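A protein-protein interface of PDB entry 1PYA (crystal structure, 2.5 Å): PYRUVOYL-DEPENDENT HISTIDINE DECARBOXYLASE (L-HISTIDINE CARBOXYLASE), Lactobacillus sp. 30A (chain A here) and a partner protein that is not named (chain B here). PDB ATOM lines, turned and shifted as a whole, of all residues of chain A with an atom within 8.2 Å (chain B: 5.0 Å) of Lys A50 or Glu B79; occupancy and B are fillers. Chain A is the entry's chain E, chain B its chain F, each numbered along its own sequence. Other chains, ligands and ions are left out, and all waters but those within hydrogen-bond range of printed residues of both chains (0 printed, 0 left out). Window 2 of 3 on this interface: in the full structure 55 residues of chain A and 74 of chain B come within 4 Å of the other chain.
Printed residues of chain A within 4 Å of Glu B79: Lys A50.
No residue of chain A comes within 4 Å of Ala B78.
Of the printed residues of chain A, Ile B172 touches Val A47, Arg A48 and Asp A57.
Of the printed residues of chain B, Arg A48 touches Gln B171 and Ile B172.
Of the printed residues of chain B, Asp A49 touches Gly B170 (3.6 Å) and Gln B171 (3.5 Å).
The nearest printed residue of chain A that does not touch Gly B170 is Arg A48 (4.6 Å).
Of the 12 printed residues of chain A, 5 touch a printed residue of chain B.
Printed residues of chain B that touch a printed residue of chain A: Glu B79, Gly B170, Gln B171 and Ile B172.
Hydrophobic or aromatic side chains of chain B that line the printed part of chain A: Ile B172.
Along chain B the printed residues that touch a printed residue of chain A span positions 79 to 172.
Among the printed residues, no Asp or Glu carboxylate lies within 4 Å of a Lys or Arg side-chain nitrogen of the other chain.
The side-chain carboxylate (OD2) of Asp A57 is in salt-bridge range of the side-chain amino group (NZ) of Lys A50 (2.8 Å).
The backbone NH (N) of Gly B92 sits at hydrogen-bond distance from the backbone carbonyl oxygen (O) of Glu B79, at 3.1 Å.
The side-chain amino group of Lys A50 is in salt-bridge range of the side-chain carboxylate of Asp A54, 2.7 Å away.
The backbone carbonyl oxygen of Gly B90 lies within hydrogen-bond range of the backbone NH of Glu B79 (3.2 Å).
OG of Ser A51 is in hydrogen-bond range of OD1 of Asp A57 (2.9 Å).
NH2 of Arg A48 lies within salt-bridge range of OD1 of Asp A57, 3.0 Å away.
The backbone carbonyl oxygen of Arg A48 sits at hydrogen-bond distance from the backbone NH of Ile B172 (2.8 Å).
The side-chain amide nitrogen (NE2) of Gln B171 sits at hydrogen-bond distance from the side-chain carboxylate (OD1) of Asp A49, 3.5 Å away.
The backbone NH (N) of Lys A50 is in hydrogen-bond range of the backbone carbonyl oxygen (O) of Gly B170 (3.0 Å).
Among the printed residues, pairs that only touch across the chains: Val A47 with Gln B171 (3.7 Å), Val A47 with Ile B172 (3.1 Å), Arg A48 with Gln B171 (3.4 Å), Asp A49 with Gly B170 (3.6 Å), Lys A50 with Glu B79 (3.4 Å) and Asp A57 with Ile B172 (3.8 Å).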
ATOM      1  N   VAL A  47      16.707  11.442 -21.312  1.00  0.00           N
ATOM      2  CA  VAL A  47      17.256  10.584 -20.257  1.00  0.00           C
ATOM      3  C   VAL A  47      16.743   9.151 -20.387  1.00  0.00           C
ATOM      4  O   VAL A  47      15.748   8.892 -21.070  1.00  0.00           O
ATOM      5  CB  VAL A  47      16.898  11.087 -18.796  1.00  0.00           C
ATOM      6  CG1 VAL A  47      17.317  12.550 -18.556  1.00  0.00           C
ATOM      7  CG2 VAL A  47      15.414  10.944 -18.594  1.00  0.00           C
ATOM      8  N   ARG A  48      17.448   8.215 -19.759  1.00  0.00           N
ATOM      9  CA  ARG A  48      17.026   6.826 -19.592  1.00  0.00           C
ATOM     10  C   ARG A  48      17.538   6.403 -18.206  1.00  0.00           C
ATOM     11  O   ARG A  48      18.509   6.988 -17.698  1.00  0.00           O
ATOM     12  CB  ARG A  48      17.624   5.995 -20.745  1.00  0.00           C
ATOM     13  CG  ARG A  48      17.979   4.516 -20.593  1.00  0.00           C
ATOM     14  CD  ARG A  48      17.139   3.312 -21.040  1.00  0.00           C
ATOM     15  NE  ARG A  48      18.186   2.360 -21.367  1.00  0.00           N
ATOM     16  CZ  ARG A  48      18.096   1.112 -21.828  1.00  0.00           C
ATOM     17  NH1 ARG A  48      16.972   0.425 -21.953  1.00  0.00           N
ATOM     18  NH2 ARG A  48      19.243   0.504 -22.128  1.00  0.00           N
ATOM     19  N   ASP A  49      16.895   5.479 -17.484  1.00  0.00           N
ATOM     20  CA  ASP A  49      17.470   4.979 -16.236  1.00  0.00           C
ATOM     21  C   ASP A  49      18.643   4.070 -16.611  1.00  0.00           C
ATOM     22  O   ASP A  49      18.565   3.312 -17.599  1.00  0.00           O
ATOM     23  CB  ASP A  49      16.469   4.167 -15.467  1.00  0.00           C
ATOM     24  CG  ASP A  49      15.208   4.910 -15.038  1.00  0.00           C
ATOM     25  OD1 ASP A  49      15.236   6.114 -14.755  1.00  0.00           O
ATOM     26  OD2 ASP A  49      14.173   4.251 -14.990  1.00  0.00           O
ATOM     27  N   LYS A  50      19.735   4.126 -15.837  1.00  0.00           N
ATOM     28  CA  LYS A  50      20.940   3.374 -16.145  1.00  0.00           C
ATOM     29  C   LYS A  50      20.766   1.877 -16.125  1.00  0.00           C
ATOM     30  O   LYS A  50      20.127   1.338 -15.227  1.00  0.00           O
ATOM     31  CB  LYS A  50      22.054   3.698 -15.177  1.00  0.00           C
ATOM     32  CG  LYS A  50      23.132   4.252 -16.070  1.00  0.00           C
ATOM     33  CD  LYS A  50      24.502   3.627 -15.816  1.00  0.00           C
ATOM     34  CE  LYS A  50      25.421   3.983 -17.003  1.00  0.00           C
ATOM     35  NZ  LYS A  50      25.390   2.932 -18.013  1.00  0.00           N
ATOM     36  N   SER A  51      21.274   1.186 -17.132  1.00  0.00           N
ATOM     37  CA  SER A  51      21.216  -0.260 -17.150  1.00  0.00           C
ATOM     38  C   SER A  51      22.674  -0.682 -17.054  1.00  0.00           C
ATOM     39  O   SER A  51      23.601   0.118 -16.995  1.00  0.00           O
ATOM     40  CB  SER A  51      20.627  -0.783 -18.463  1.00  0.00           C
ATOM     41  OG  SER A  51      21.587  -0.696 -19.543  1.00  0.00           O
ATOM     42  N   ASP A  52      22.838  -1.989 -17.147  1.00  0.00           N
ATOM     43  CA  ASP A  52      24.122  -2.670 -17.267  1.00  0.00           C
ATOM     44  C   ASP A  52      24.922  -2.218 -18.501  1.00  0.00           C
ATOM     45  O   ASP A  52      26.135  -2.395 -18.534  1.00  0.00           O
ATOM     46  CB  ASP A  52      23.852  -4.212 -17.348  1.00  0.00           C
ATOM     47  CG  ASP A  52      22.670  -4.610 -18.273  1.00  0.00           C
ATOM     48  OD1 ASP A  52      22.618  -4.216 -19.440  1.00  0.00           O
ATOM     49  OD2 ASP A  52      21.751  -5.293 -17.822  1.00  0.00           O
ATOM     50  N   ASP A  53      24.288  -1.668 -19.547  1.00  0.00           N
ATOM     51  CA  ASP A  53      24.930  -1.437 -20.825  1.00  0.00           C
ATOM     52  C   ASP A  53      24.965   0.014 -21.283  1.00  0.00           C
ATOM     53  O   ASP A  53      23.921   0.550 -21.660  1.00  0.00           O
ATOM     54  CB  ASP A  53      24.184  -2.306 -21.809  1.00  0.00           C
ATOM     55  CG  ASP A  53      24.825  -2.547 -23.157  1.00  0.00           C
ATOM     56  OD1 ASP A  53      25.407  -1.643 -23.769  1.00  0.00           O
ATOM     57  OD2 ASP A  53      24.704  -3.683 -23.599  1.00  0.00           O
ATOM     58  N   ASP A  54      26.148   0.638 -21.328  1.00  0.00           N
ATOM     59  CA  ASP A  54      26.358   2.016 -21.782  1.00  0.00           C
ATOM     60  C   ASP A  54      25.965   2.314 -23.225  1.00  0.00           C
ATOM     61  O   ASP A  54      25.381   3.360 -23.490  1.00  0.00           O
ATOM     62  CB  ASP A  54      27.808   2.430 -21.677  1.00  0.00           C
ATOM     63  CG  ASP A  54      28.393   2.425 -20.276  1.00  0.00           C
ATOM     64  OD1 ASP A  54      27.678   2.174 -19.314  1.00  0.00           O
ATOM     65  OD2 ASP A  54      29.589   2.671 -20.141  1.00  0.00           O
ATOM     66  N   VAL A  55      26.247   1.433 -24.172  1.00  0.00           N
ATOM     67  CA  VAL A  55      25.914   1.671 -25.553  1.00  0.00           C
ATOM     68  C   VAL A  55      24.406   1.814 -25.698  1.00  0.00           C
ATOM     69  O   VAL A  55      23.951   2.800 -26.298  1.00  0.00           O
ATOM     70  CB  VAL A  55      26.474   0.508 -26.389  1.00  0.00           C
ATOM     71  CG1 VAL A  55      26.038   0.634 -27.826  1.00  0.00           C
ATOM     72  CG2 VAL A  55      28.000   0.535 -26.333  1.00  0.00           C
ATOM     73  N   LEU A  56      23.647   0.915 -25.050  1.00  0.00           N
ATOM     74  CA  LEU A  56      22.206   0.892 -25.139  1.00  0.00           C
ATOM     75  C   LEU A  56      21.587   2.053 -24.421  1.00  0.00           C
ATOM     76  O   LEU A  56      20.614   2.619 -24.904  1.00  0.00           O
ATOM     77  CB  LEU A  56      21.649  -0.436 -24.583  1.00  0.00           C
ATOM     78  CG  LEU A  56      22.001  -1.685 -25.391  1.00  0.00           C
ATOM     79  CD1 LEU A  56      21.398  -2.899 -24.715  1.00  0.00           C
ATOM     80  CD2 LEU A  56      21.479  -1.570 -26.811  1.00  0.00           C
ATOM     81  N   ASP A  57      22.183   2.454 -23.304  1.00  0.00           N
ATOM     82  CA  ASP A  57      21.746   3.620 -22.571  1.00  0.00           C
ATOM     83  C   ASP A  57      21.943   4.848 -23.430  1.00  0.00           C
ATOM     84  O   ASP A  57      21.010   5.654 -23.512  1.00  0.00           O
ATOM     85  CB  ASP A  57      22.547   3.745 -21.270  1.00  0.00           C
ATOM     86  CG  ASP A  57      22.137   2.748 -20.187  1.00  0.00           C
ATOM     87  OD1 ASP A  57      21.103   2.074 -20.319  1.00  0.00           O
ATOM     88  OD2 ASP A  57      22.856   2.655 -19.197  1.00  0.00           O
ATOM     89  N   GLY A  58      23.094   4.993 -24.083  1.00  0.00           N
ATOM     90  CA  GLY A  58      23.356   6.095 -24.991  1.00  0.00           C
ATOM     91  C   GLY A  58      22.387   6.084 -26.175  1.00  0.00           C
ATOM     92  O   GLY A  58      21.909   7.160 -26.559  1.00  0.00           O
ATOM     93  N   THR B  77      26.909  12.535 -23.128  1.00  0.00           N
ATOM     94  CA  THR B  77      26.181  11.750 -22.138  1.00  0.00           C
ATOM     95  C   THR B  77      26.910  11.849 -20.807  1.00  0.00           C
ATOM     96  O   THR B  77      28.139  12.049 -20.764  1.00  0.00           O
ATOM     97  CB  THR B  77      26.082  10.261 -22.545  1.00  0.00           C
ATOM     98  OG1 THR B  77      27.379   9.870 -22.959  1.00  0.00           O
ATOM     99  CG2 THR B  77      25.168   9.988 -23.710  1.00  0.00           C
ATOM    100  N   ALA B  78      26.191  11.687 -19.704  1.00  0.00           N
ATOM    101  CA  ALA B  78      26.771  11.599 -18.373  1.00  0.00           C
ATOM    102  C   ALA B  78      25.744  10.812 -17.591  1.00  0.00           C
ATOM    103  O   ALA B  78      24.543  10.818 -17.898  1.00  0.00           O
ATOM    104  CB  ALA B  78      26.904  12.939 -17.657  1.00  0.00           C
ATOM    105  N   GLU B  79      26.245  10.142 -16.564  1.00  0.00           N
ATOM    106  CA  GLU B  79      25.427   9.361 -15.657  1.00  0.00           C
ATOM    107  C   GLU B  79      25.393   9.964 -14.248  1.00  0.00           C
ATOM    108  O   GLU B  79      26.439  10.418 -13.757  1.00  0.00           O
ATOM    109  CB  GLU B  79      26.034   7.964 -15.667  1.00  0.00           C
ATOM    110  CG  GLU B  79      25.571   7.063 -14.538  1.00  0.00           C
ATOM    111  CD  GLU B  79      26.546   5.969 -14.114  1.00  0.00           C
ATOM    112  OE1 GLU B  79      27.676   5.914 -14.602  1.00  0.00           O
ATOM    113  OE2 GLU B  79      26.153   5.156 -13.279  1.00  0.00           O
ATOM    114  N   ARG B  80      24.245  10.022 -13.589  1.00  0.00           N
ATOM    115  CA  ARG B  80      24.179  10.369 -12.171  1.00  0.00           C
ATOM    116  C   ARG B  80      24.092   8.999 -11.466  1.00  0.00           C
ATOM    117  O   ARG B  80      23.169   8.204 -11.763  1.00  0.00           O
ATOM    118  CB  ARG B  80      22.912  11.152 -11.781  1.00  0.00           C
ATOM    119  CG  ARG B  80      23.285  12.341 -10.941  1.00  0.00           C
ATOM    120  CD  ARG B  80      22.851  12.391  -9.491  1.00  0.00           C
ATOM    121  NE  ARG B  80      21.572  13.059  -9.329  1.00  0.00           N
ATOM    122  CZ  ARG B  80      21.147  13.452  -8.115  1.00  0.00           C
ATOM    123  NH1 ARG B  80      21.839  13.251  -6.996  1.00  0.00           N
ATOM    124  NH2 ARG B  80      19.988  14.068  -7.983  1.00  0.00           N
ATOM    125  N   PRO B  81      24.995   8.633 -10.539  1.00  0.00           N
ATOM    126  CA  PRO B  81      24.888   7.432  -9.696  1.00  0.00           C
ATOM    127  C   PRO B  81      23.624   7.253  -8.864  1.00  0.00           C
ATOM    128  O   PRO B  81      22.978   8.234  -8.473  1.00  0.00           O
ATOM    129  CB  PRO B  81      26.111   7.499  -8.869  1.00  0.00           C
ATOM    130  CG  PRO B  81      26.500   8.940  -8.925  1.00  0.00           C
ATOM    131  CD  PRO B  81      26.281   9.265 -10.365  1.00  0.00           C
ATOM    132  N   GLY B  90      32.955   9.772 -15.976  1.00  0.00           N
ATOM    133  CA  GLY B  90      31.896  10.144 -16.937  1.00  0.00           C
ATOM    134  C   GLY B  90      30.560  10.512 -16.278  1.00  0.00           C
ATOM    135  O   GLY B  90      29.465  10.156 -16.806  1.00  0.00           O
ATOM    136  N   GLN B  91      30.643  11.212 -15.135  1.00  0.00           N
ATOM    137  CA  GLN B  91      29.473  11.374 -14.303  1.00  0.00           C
ATOM    138  C   GLN B  91      29.193  12.791 -13.893  1.00  0.00           C
ATOM    139  O   GLN B  91      30.127  13.584 -13.821  1.00  0.00           O
ATOM    140  CB  GLN B  91      29.622  10.540 -13.066  1.00  0.00           C
ATOM    141  CG  GLN B  91      29.410   9.037 -13.248  1.00  0.00           C
ATOM    142  CD  GLN B  91      29.676   8.186 -12.008  1.00  0.00           C
ATOM    143  OE1 GLN B  91      30.205   8.597 -10.973  1.00  0.00           O
ATOM    144  NE2 GLN B  91      29.341   6.921 -12.108  1.00  0.00           N
ATOM    145  N   GLY B  92      27.927  13.124 -13.606  1.00  0.00           N
ATOM    146  CA  GLY B  92      27.611  14.468 -13.225  1.00  0.00           C
ATOM    147  C   GLY B  92      26.190  14.572 -12.850  1.00  0.00           C
ATOM    148  O   GLY B  92      25.481  13.573 -12.843  1.00  0.00           O
ATOM    149  N   MET B 167      19.751  15.239 -14.053  1.00  0.00           N
ATOM    150  CA  MET B 167      19.393  13.841 -13.857  1.00  0.00           C
ATOM    151  C   MET B 167      18.950  13.525 -12.441  1.00  0.00           C
ATOM    152  O   MET B 167      19.484  14.061 -11.457  1.00  0.00           O
ATOM    153  CB  MET B 167      20.573  12.914 -14.176  1.00  0.00           C
ATOM    154  CG  MET B 167      20.950  12.709 -15.647  1.00  0.00           C
ATOM    155  SD  MET B 167      21.954  14.049 -16.310  1.00  0.00           S
ATOM    156  CE  MET B 167      23.522  13.453 -15.758  1.00  0.00           C
ATOM    157  N   GLY B 170      20.793   7.674 -10.651  1.00  0.00           N
ATOM    158  CA  GLY B 170      20.702   6.479 -11.471  1.00  0.00           C
ATOM    159  C   GLY B 170      20.108   6.703 -12.853  1.00  0.00           C
ATOM    160  O   GLY B 170      19.474   5.786 -13.395  1.00  0.00           O
ATOM    161  N   GLN B 171      20.287   7.889 -13.446  1.00  0.00           N
ATOM    162  CA  GLN B 171      19.792   8.163 -14.777  1.00  0.00           C
ATOM    163  C   GLN B 171      20.957   8.570 -15.618  1.00  0.00           C
ATOM    164  O   GLN B 171      21.936   9.127 -15.095  1.00  0.00           O
ATOM    165  CB  GLN B 171      18.828   9.313 -14.842  1.00  0.00           C
ATOM    166  CG  GLN B 171      17.509   9.027 -14.194  1.00  0.00           C
ATOM    167  CD  GLN B 171      16.445  10.012 -14.629  1.00  0.00           C
ATOM    168  OE1 GLN B 171      16.547  11.214 -14.470  1.00  0.00           O
ATOM    169  NE2 GLN B 171      15.352   9.548 -15.201  1.00  0.00           N
ATOM    170  N   ILE B 172      20.884   8.270 -16.894  1.00  0.00           N
ATOM    171  CA  ILE B 172      21.869   8.764 -17.841  1.00  0.00           C
ATOM    172  C   ILE B 172      21.181   9.828 -18.716  1.00  0.00           C
ATOM    173  O   ILE B 172      20.023   9.680 -19.154  1.00  0.00           O
ATOM    174  CB  ILE B 172      22.441   7.608 -18.694  1.00  0.00           C
ATOM    175  CG1 ILE B 172      23.531   8.239 -19.575  1.00  0.00           C
ATOM    176  CG2 ILE B 172      21.364   6.868 -19.478  1.00  0.00           C
ATOM    177  CD1 ILE B 172      24.111   7.481 -20.794  1.00  0.00           C
